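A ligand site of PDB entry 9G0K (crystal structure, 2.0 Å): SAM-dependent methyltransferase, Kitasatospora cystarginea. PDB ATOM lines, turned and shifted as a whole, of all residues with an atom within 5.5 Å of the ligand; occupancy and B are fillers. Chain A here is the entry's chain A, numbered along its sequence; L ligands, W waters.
O of Leu 105 lies close to S1 of the ligand (3.6 Å).
Merely in contact with the ligand: Gly 42 (3.4 Å), Ser 65 (3.8 Å), Met 68 (3.6 Å), Ala 87 (3.8 Å), His 109 (3.8 Å) and Leu 110 (3.7 Å).
Hydrophobic or aromatic side chains within 4 Å of the ligand: Tyr 19, Met 68, His 89, Ala 104, His 109 and Leu 110.
Of the 25 residues printed, 16 come within 4 Å of the ligand.
The nearest printed residue that does not touch the ligand is Leu 45 (4.1 Å).
OG of Ser 106 is in hydrogen-bond range of NE2 of His 89 (2.7 Å).
The backbone NH (N) of Gly 42 lies within hydrogen-bond range of the side-chain carboxylate (OD1) of Asp 63 (2.6 Å).
OD2 of Asp 63 lies within hydrogen-bond range of N of Ser 65, at 3.1 Å.
The backbone carbonyl oxygen (O) of Asp 63 sits at hydrogen-bond distance from the backbone NH (N) of Ala 87 (3.2 Å).
OD1 of Asp 88 is in salt-bridge range of NH1 of Arg 64 (3.4 Å).
The side-chain carboxylate of Asp 88 sits at hydrogen-bond distance from the backbone NH of Leu 90 (3.0 Å).
The backbone NH (N) of Arg 64 sits at hydrogen-bond distance from the backbone carbonyl oxygen (O) of Ala 87, 3.1 Å away.
The backbone NH (N) of Met 68 sits at hydrogen-bond distance from the side-chain hydroxyl (OG) of Ser 65 (3.1 Å).
Water W2 lies within hydrogen-bond range of the backbone carbonyl oxygen of Ala 41, the side-chain carboxylate of Asp 38, a nitrogen (N1) of the ligand and the backbone NH of Leu 46.
The side-chain hydroxyl (OH) of Tyr 19 is in hydrogen-bond range of an oxygen (O1) of the ligand, 2.6 Å away.
O3 of the ligand is in hydrogen-bond range of OG of Ser 106, 2.8 Å away.
An oxygen (O4) of the ligand sits at hydrogen-bond distance from the side-chain carboxylate (OD1) of Asp 63, 2.8 Å away.
The backbone NH (N) of His 89 sits at hydrogen-bond distance from a nitrogen (N5) of the ligand, 2.9 Å away.
A nitrogen (N5) of the ligand lies close to a ring nitrogen (ND1) of His 89, at 3.5 Å.
The side-chain carboxylate (OD2) of Asp 88 lies within hydrogen-bond range of a nitrogen (N4) of the ligand, at 2.9 Å.
O of Ala 41 sits close to N1 of the ligand.
The backbone carbonyl oxygen (O) of Gly 40 lies within hydrogen-bond range of a nitrogen (N1) of the ligand, 3.2 Å away.
The backbone carbonyl oxygen (O) of Ala 104 sits at hydrogen-bond distance from a nitrogen (N1) of the ligand (3.2 Å).
The backbone NH of Arg 64 lies within hydrogen-bond range of a nitrogen (N6) of the ligand, 3.4 Å away.
The guanidinium group of Arg 64 sits close to a nitrogen (N3) of the ligand (3.5 Å).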
ATOM      1  N   TYR A   4     -33.472 -38.955  14.974  1.00  0.00           N
ATOM      2  CA  TYR A   4     -33.264 -37.921  16.030  1.00  0.00           C
ATOM      3  C   TYR A   4     -33.733 -36.563  15.522  1.00  0.00           C
ATOM      4  O   TYR A   4     -34.403 -35.847  16.285  1.00  0.00           O
ATOM      5  CB  TYR A   4     -31.813 -37.830  16.522  1.00  0.00           C
ATOM      6  CG  TYR A   4     -31.673 -37.064  17.814  1.00  0.00           C
ATOM      7  CD1 TYR A   4     -31.562 -37.708  19.030  1.00  0.00           C
ATOM      8  CD2 TYR A   4     -31.704 -35.663  17.831  1.00  0.00           C
ATOM      9  CE1 TYR A   4     -31.466 -37.005  20.227  1.00  0.00           C
ATOM     10  CE2 TYR A   4     -31.614 -34.950  19.020  1.00  0.00           C
ATOM     11  CZ  TYR A   4     -31.490 -35.622  20.227  1.00  0.00           C
ATOM     12  OH  TYR A   4     -31.366 -34.923  21.410  1.00  0.00           O
ATOM     13  N   ARG A   8     -36.939 -34.080  17.069  1.00  0.00           N
ATOM     14  CA  ARG A   8     -36.794 -32.673  17.547  1.00  0.00           C
ATOM     15  C   ARG A   8     -37.897 -31.820  16.913  1.00  0.00           C
ATOM     16  O   ARG A   8     -38.480 -30.971  17.609  1.00  0.00           O
ATOM     17  CB  ARG A   8     -35.383 -32.148  17.276  1.00  0.00           C
ATOM     18  CG  ARG A   8     -34.289 -32.879  18.037  1.00  0.00           C
ATOM     19  CD  ARG A   8     -34.616 -33.138  19.492  1.00  0.00           C
ATOM     20  NE  ARG A   8     -34.564 -31.912  20.282  1.00  0.00           N
ATOM     21  CZ  ARG A   8     -34.849 -31.825  21.575  1.00  0.00           C
ATOM     22  NH1 ARG A   8     -35.224 -32.894  22.260  1.00  0.00           N
ATOM     23  NH2 ARG A   8     -34.777 -30.662  22.194  1.00  0.00           N
ATOM     24  N   TYR A  19     -35.453 -22.035  14.326  1.00  0.00           N
ATOM     25  CA  TYR A  19     -34.063 -22.378  13.972  1.00  0.00           C
ATOM     26  C   TYR A  19     -33.607 -21.522  12.804  1.00  0.00           C
ATOM     27  O   TYR A  19     -32.457 -20.916  12.916  1.00  0.00           O
ATOM     28  CB  TYR A  19     -33.877 -23.863  13.703  1.00  0.00           C
ATOM     29  CG  TYR A  19     -33.565 -24.603  14.990  1.00  0.00           C
ATOM     30  CD1 TYR A  19     -32.307 -25.077  15.264  1.00  0.00           C
ATOM     31  CD2 TYR A  19     -34.562 -24.919  15.878  1.00  0.00           C
ATOM     32  CE1 TYR A  19     -32.033 -25.791  16.415  1.00  0.00           C
ATOM     33  CE2 TYR A  19     -34.310 -25.569  17.057  1.00  0.00           C
ATOM     34  CZ  TYR A  19     -33.046 -26.050  17.316  1.00  0.00           C
ATOM     35  OH  TYR A  19     -32.793 -26.773  18.442  1.00  0.00           O
ATOM     36  N   ASP A  38     -20.934 -22.631  19.097  1.00  0.00           N
ATOM     37  CA  ASP A  38     -22.268 -23.222  19.403  1.00  0.00           C
ATOM     38  C   ASP A  38     -22.232 -23.775  20.831  1.00  0.00           C
ATOM     39  O   ASP A  38     -21.579 -24.819  21.037  1.00  0.00           O
ATOM     40  CB  ASP A  38     -22.677 -24.276  18.368  1.00  0.00           C
ATOM     41  CG  ASP A  38     -24.118 -24.722  18.493  1.00  0.00           C
ATOM     42  OD1 ASP A  38     -24.879 -24.066  19.229  1.00  0.00           O
ATOM     43  OD2 ASP A  38     -24.476 -25.727  17.862  1.00  0.00           O
ATOM     44  N   LEU A  39     -22.898 -23.105  21.769  1.00  0.00           N
ATOM     45  CA  LEU A  39     -22.913 -23.442  23.206  1.00  0.00           C
ATOM     46  C   LEU A  39     -24.034 -24.415  23.465  1.00  0.00           C
ATOM     47  O   LEU A  39     -25.214 -24.015  23.134  1.00  0.00           O
ATOM     48  CB  LEU A  39     -23.219 -22.214  24.075  1.00  0.00           C
ATOM     49  CG  LEU A  39     -22.075 -21.271  24.318  1.00  0.00           C
ATOM     50  CD1 LEU A  39     -22.568 -20.171  25.260  1.00  0.00           C
ATOM     51  CD2 LEU A  39     -20.818 -22.014  24.896  1.00  0.00           C
ATOM     52  N   GLY A  40     -23.677 -25.500  24.163  1.00  0.00           N
ATOM     53  CA  GLY A  40     -24.555 -26.662  24.329  1.00  0.00           C
ATOM     54  C   GLY A  40     -25.147 -27.117  23.007  1.00  0.00           C
ATOM     55  O   GLY A  40     -26.296 -27.327  22.972  1.00  0.00           O
ATOM     56  N   ALA A  41     -24.277 -27.406  22.022  1.00  0.00           N
ATOM     57  CA  ALA A  41     -24.695 -27.801  20.663  1.00  0.00           C
ATOM     58  C   ALA A  41     -25.336 -29.195  20.614  1.00  0.00           C
ATOM     59  O   ALA A  41     -26.070 -29.465  19.636  1.00  0.00           O
ATOM     60  CB  ALA A  41     -23.487 -27.753  19.771  1.00  0.00           C
ATOM     61  N   GLY A  42     -25.048 -30.065  21.588  1.00  0.00           N
ATOM     62  CA  GLY A  42     -25.594 -31.433  21.583  1.00  0.00           C
ATOM     63  C   GLY A  42     -25.184 -32.202  20.329  1.00  0.00           C
ATOM     64  O   GLY A  42     -23.973 -32.286  20.063  1.00  0.00           O
ATOM     65  N   THR A  43     -26.160 -32.755  19.595  1.00  0.00           N
ATOM     66  CA  THR A  43     -25.863 -33.455  18.325  1.00  0.00           C
ATOM     67  C   THR A  43     -25.541 -32.444  17.225  1.00  0.00           C
ATOM     68  O   THR A  43     -25.261 -32.896  16.118  1.00  0.00           O
ATOM     69  CB  THR A  43     -27.048 -34.299  17.852  1.00  0.00           C
ATOM     70  OG1 THR A  43     -28.088 -33.379  17.517  1.00  0.00           O
ATOM     71  CG2 THR A  43     -27.516 -35.319  18.879  1.00  0.00           C
ATOM     72  N   GLY A  44     -25.595 -31.140  17.526  1.00  0.00           N
ATOM     73  CA  GLY A  44     -25.043 -30.088  16.639  1.00  0.00           C
ATOM     74  C   GLY A  44     -25.992 -29.761  15.493  1.00  0.00           C
ATOM     75  O   GLY A  44     -25.524 -29.413  14.389  1.00  0.00           O
ATOM     76  N   LEU A  45     -27.287 -29.763  15.782  1.00  0.00           N
ATOM     77  CA  LEU A  45     -28.335 -29.430  14.786  1.00  0.00           C
ATOM     78  C   LEU A  45     -28.231 -27.941  14.394  1.00  0.00           C
ATOM     79  O   LEU A  45     -28.382 -27.642  13.205  1.00  0.00           O
ATOM     80  CB  LEU A  45     -29.688 -29.746  15.426  1.00  0.00           C
ATOM     81  CG  LEU A  45     -30.858 -29.964  14.458  1.00  0.00           C
ATOM     82  CD1 LEU A  45     -30.477 -30.943  13.359  1.00  0.00           C
ATOM     83  CD2 LEU A  45     -32.073 -30.453  15.218  1.00  0.00           C
ATOM     84  N   LEU A  46     -28.015 -27.058  15.378  1.00  0.00           N
ATOM     85  CA  LEU A  46     -27.944 -25.602  15.045  1.00  0.00           C
ATOM     86  C   LEU A  46     -26.680 -25.341  14.220  1.00  0.00           C
ATOM     87  O   LEU A  46     -26.787 -24.641  13.175  1.00  0.00           O
ATOM     88  CB  LEU A  46     -27.971 -24.762  16.303  1.00  0.00           C
ATOM     89  CG  LEU A  46     -27.981 -23.249  16.061  1.00  0.00           C
ATOM     90  CD1 LEU A  46     -29.086 -22.798  15.114  1.00  0.00           C
ATOM     91  CD2 LEU A  46     -28.068 -22.508  17.386  1.00  0.00           C
ATOM     92  N   ASP A  63     -19.992 -28.545  24.438  1.00  0.00           N
ATOM     93  CA  ASP A  63     -21.098 -29.147  25.235  1.00  0.00           C
ATOM     94  C   ASP A  63     -20.477 -29.926  26.375  1.00  0.00           C
ATOM     95  O   ASP A  63     -19.378 -30.438  26.142  1.00  0.00           O
ATOM     96  CB  ASP A  63     -21.911 -30.058  24.313  1.00  0.00           C
ATOM     97  CG  ASP A  63     -23.296 -30.360  24.824  1.00  0.00           C
ATOM     98  OD1 ASP A  63     -24.263 -30.027  24.113  1.00  0.00           O
ATOM     99  OD2 ASP A  63     -23.361 -30.928  25.921  1.00  0.00           O
ATOM    100  N   ARG A  64     -21.168 -30.095  27.514  1.00  0.00           N
ATOM    101  CA  ARG A  64     -20.566 -30.896  28.651  1.00  0.00           C
ATOM    102  C   ARG A  64     -20.616 -32.402  28.375  1.00  0.00           C
ATOM    103  O   ARG A  64     -19.813 -33.128  28.979  1.00  0.00           O
ATOM    104  CB  ARG A  64     -21.171 -30.580  30.033  1.00  0.00           C
ATOM    105  CG  ARG A  64     -22.613 -30.993  30.217  1.00  0.00           C
ATOM    106  CD  ARG A  64     -23.054 -30.549  31.572  1.00  0.00           C
ATOM    107  NE  ARG A  64     -24.488 -30.782  31.778  1.00  0.00           N
ATOM    108  CZ  ARG A  64     -25.156 -30.355  32.842  1.00  0.00           C
ATOM    109  NH1 ARG A  64     -24.523 -29.656  33.792  1.00  0.00           N
ATOM    110  NH2 ARG A  64     -26.438 -30.637  32.967  1.00  0.00           N
ATOM    111  N   SER A  65     -21.509 -32.849  27.485  1.00  0.00           N
ATOM    112  CA  SER A  65     -21.753 -34.289  27.211  1.00  0.00           C
ATOM    113  C   SER A  65     -20.940 -34.766  26.003  1.00  0.00           C
ATOM    114  O   SER A  65     -21.315 -34.455  24.870  1.00  0.00           O
ATOM    115  CB  SER A  65     -23.209 -34.575  26.997  1.00  0.00           C
ATOM    116  OG  SER A  65     -23.396 -35.908  26.535  1.00  0.00           O
ATOM    117  N   MET A  68     -23.123 -36.659  23.512  1.00  0.00           N
ATOM    118  CA  MET A  68     -23.891 -35.787  22.576  1.00  0.00           C
ATOM    119  C   MET A  68     -22.937 -35.324  21.475  1.00  0.00           C
ATOM    120  O   MET A  68     -23.276 -35.518  20.272  1.00  0.00           O
ATOM    121  CB  MET A  68     -24.521 -34.575  23.259  1.00  0.00           C
ATOM    122  CG  MET A  68     -25.628 -34.922  24.256  1.00  0.00           C
ATOM    123  SD  MET A  68     -27.098 -35.659  23.497  1.00  0.00           S
ATOM    124  CE  MET A  68     -27.757 -34.273  22.560  1.00  0.00           C
ATOM    125  N   ALA A  87     -16.840 -28.992  27.354  1.00  0.00           N
ATOM    126  CA  ALA A  87     -16.800 -27.950  28.416  1.00  0.00           C
ATOM    127  C   ALA A  87     -18.204 -27.702  28.981  1.00  0.00           C
ATOM    128  O   ALA A  87     -19.161 -27.806  28.196  1.00  0.00           O
ATOM    129  CB  ALA A  87     -16.231 -26.710  27.782  1.00  0.00           C
ATOM    130  N   ASP A  88     -18.296 -27.396  30.274  1.00  0.00           N
ATOM    131  CA  ASP A  88     -19.537 -26.849  30.906  1.00  0.00           C
ATOM    132  C   ASP A  88     -19.643 -25.353  30.553  1.00  0.00           C
ATOM    133  O   ASP A  88     -18.625 -24.700  30.365  1.00  0.00           O
ATOM    134  CB  ASP A  88     -19.553 -27.186  32.412  1.00  0.00           C
ATOM    135  CG  ASP A  88     -20.932 -27.102  33.075  1.00  0.00           C
ATOM    136  OD1 ASP A  88     -21.406 -28.194  33.617  1.00  0.00           O
ATOM    137  OD2 ASP A  88     -21.534 -25.957  33.065  1.00  0.00           O
ATOM    138  N   HIS A  89     -20.864 -24.831  30.399  1.00  0.00           N
ATOM    139  CA  HIS A  89     -21.171 -23.378  30.288  1.00  0.00           C
ATOM    140  C   HIS A  89     -20.468 -22.648  31.442  1.00  0.00           C
ATOM    141  O   HIS A  89     -20.052 -21.507  31.270  1.00  0.00           O
ATOM    142  CB  HIS A  89     -22.679 -23.096  30.326  1.00  0.00           C
ATOM    143  CG  HIS A  89     -23.501 -23.675  29.222  1.00  0.00           C
ATOM    144  ND1 HIS A  89     -22.970 -24.070  28.028  1.00  0.00           N
ATOM    145  CD2 HIS A  89     -24.854 -23.840  29.112  1.00  0.00           C
ATOM    146  CE1 HIS A  89     -23.942 -24.511  27.234  1.00  0.00           C
ATOM    147  NE2 HIS A  89     -25.123 -24.352  27.849  1.00  0.00           N
ATOM    148  N   LEU A  90     -20.333 -23.271  32.602  1.00  0.00           N
ATOM    149  CA  LEU A  90     -19.740 -22.572  33.797  1.00  0.00           C
ATOM    150  C   LEU A  90     -18.211 -22.569  33.783  1.00  0.00           C
ATOM    151  O   LEU A  90     -17.647 -21.840  34.602  1.00  0.00           O
ATOM    152  CB  LEU A  90     -20.289 -23.276  35.024  1.00  0.00           C
ATOM    153  CG  LEU A  90     -21.793 -23.100  35.096  1.00  0.00           C
ATOM    154  CD1 LEU A  90     -22.480 -24.300  35.758  1.00  0.00           C
ATOM    155  CD2 LEU A  90     -22.121 -21.789  35.792  1.00  0.00           C
ATOM    156  N   ALA A 104     -29.052 -23.225  21.352  1.00  0.00           N
ATOM    157  CA  ALA A 104     -30.428 -23.764  21.268  1.00  0.00           C
ATOM    158  C   ALA A 104     -30.682 -24.690  22.476  1.00  0.00           C
ATOM    159  O   ALA A 104     -29.956 -25.736  22.690  1.00  0.00           O
ATOM    160  CB  ALA A 104     -30.582 -24.486  19.942  1.00  0.00           C
ATOM    161  N   LEU A 105     -31.675 -24.295  23.251  1.00  0.00           N
ATOM    162  CA  LEU A 105     -32.329 -25.171  24.237  1.00  0.00           C
ATOM    163  C   LEU A 105     -31.268 -25.676  25.235  1.00  0.00           C
ATOM    164  O   LEU A 105     -31.323 -26.884  25.635  1.00  0.00           O
ATOM    165  CB  LEU A 105     -33.028 -26.314  23.474  1.00  0.00           C
ATOM    166  CG  LEU A 105     -34.037 -25.949  22.361  1.00  0.00           C
ATOM    167  CD1 LEU A 105     -34.755 -27.195  21.936  1.00  0.00           C
ATOM    168  CD2 LEU A 105     -35.061 -24.902  22.767  1.00  0.00           C
ATOM    169  N   SER A 106     -30.365 -24.810  25.716  1.00  0.00           N
ATOM    170  CA  SER A 106     -29.331 -25.244  26.688  1.00  0.00           C
ATOM    171  C   SER A 106     -29.231 -24.378  27.963  1.00  0.00           C
ATOM    172  O   SER A 106     -29.193 -24.940  29.110  1.00  0.00           O
ATOM    173  CB  SER A 106     -28.025 -25.284  26.009  1.00  0.00           C
ATOM    174  OG  SER A 106     -27.069 -25.897  26.882  1.00  0.00           O
ATOM    175  N   HIS A 109     -31.031 -24.512  31.377  1.00  0.00           N
ATOM    176  CA  HIS A 109     -30.597 -25.530  32.378  1.00  0.00           C
ATOM    177  C   HIS A 109     -29.754 -24.870  33.444  1.00  0.00           C
ATOM    178  O   HIS A 109     -29.579 -25.467  34.463  1.00  0.00           O
ATOM    179  CB  HIS A 109     -29.741 -26.659  31.824  1.00  0.00           C
ATOM    180  CG  HIS A 109     -30.500 -27.690  31.079  1.00  0.00           C
ATOM    181  ND1 HIS A 109     -30.659 -27.621  29.706  1.00  0.00           N
ATOM    182  CD2 HIS A 109     -31.096 -28.826  31.465  1.00  0.00           C
ATOM    183  CE1 HIS A 109     -31.323 -28.655  29.271  1.00  0.00           C
ATOM    184  NE2 HIS A 109     -31.622 -29.391  30.326  1.00  0.00           N
ATOM    185  N   LEU A 110     -29.333 -23.624  33.255  1.00  0.00           N
ATOM    186  CA  LEU A 110     -28.568 -22.911  34.298  1.00  0.00           C
ATOM    187  C   LEU A 110     -29.485 -22.244  35.371  1.00  0.00           C
ATOM    188  O   LEU A 110     -30.671 -21.900  35.073  1.00  0.00           O
ATOM    189  CB  LEU A 110     -27.679 -21.925  33.540  1.00  0.00           C
ATOM    190  CG  LEU A 110     -26.523 -22.560  32.742  1.00  0.00           C
ATOM    191  CD1 LEU A 110     -25.676 -21.504  32.022  1.00  0.00           C
ATOM    192  CD2 LEU A 110     -25.618 -23.380  33.658  1.00  0.00           C
HETATM  193  N1  LIG L   1     -28.377 -27.510  20.601  1.00  0.00           N
HETATM  194  C1  LIG L   1     -28.963 -28.884  20.604  1.00  0.00           C
HETATM  195  C2  LIG L   1     -28.995 -29.468  22.042  1.00  0.00           C
HETATM  196  C3  LIG L   1     -30.221 -29.162  22.860  1.00  0.00           C
HETATM  197  S1  LIG L   1     -30.240 -30.132  24.439  1.00  0.00           S
HETATM  198  C4  LIG L   1     -30.323 -28.820  19.900  1.00  0.00           C
HETATM  199  O1  LIG L   1     -30.847 -27.710  19.848  1.00  0.00           O
HETATM  200  O2  LIG L   1     -30.934 -29.728  19.280  1.00  0.00           O
HETATM  201  C5  LIG L   1     -29.240 -29.087  25.525  1.00  0.00           C
HETATM  202  C6  LIG L   1     -27.783 -29.467  25.550  1.00  0.00           C
HETATM  203  O3  LIG L   1     -27.153 -28.656  26.567  1.00  0.00           O
HETATM  204  C7  LIG L   1     -27.425 -30.926  25.881  1.00  0.00           C
HETATM  205  O4  LIG L   1     -26.569 -31.478  24.870  1.00  0.00           O
HETATM  206  C8  LIG L   1     -26.756 -30.826  27.259  1.00  0.00           C
HETATM  207  O5  LIG L   1     -25.785 -31.818  27.466  1.00  0.00           O
HETATM  208  C9  LIG L   1     -26.170 -29.417  27.225  1.00  0.00           C
HETATM  209  N2  LIG L   1     -25.990 -28.814  28.551  1.00  0.00           N
HETATM  210  C10 LIG L   1     -26.894 -28.718  29.572  1.00  0.00           C
HETATM  211  N3  LIG L   1     -26.443 -28.058  30.621  1.00  0.00           N
HETATM  212  C11 LIG L   1     -25.169 -27.682  30.261  1.00  0.00           C
HETATM  213  C12 LIG L   1     -24.155 -26.969  30.909  1.00  0.00           C
HETATM  214  N4  LIG L   1     -24.269 -26.450  32.130  1.00  0.00           N
HETATM  215  N5  LIG L   1     -23.004 -26.758  30.249  1.00  0.00           N
HETATM  216  C13 LIG L   1     -22.852 -27.282  29.032  1.00  0.00           C
HETATM  217  N6  LIG L   1     -23.725 -27.966  28.316  1.00  0.00           N
HETATM  218  C14 LIG L   1     -24.878 -28.128  28.992  1.00  0.00           C
HETATM  219  O   HOH W   1     -26.639 -25.144  21.066  1.00  0.00           O
HETATM  220  O   HOH W   2     -26.611 -27.319  18.286  1.00  0.00           O
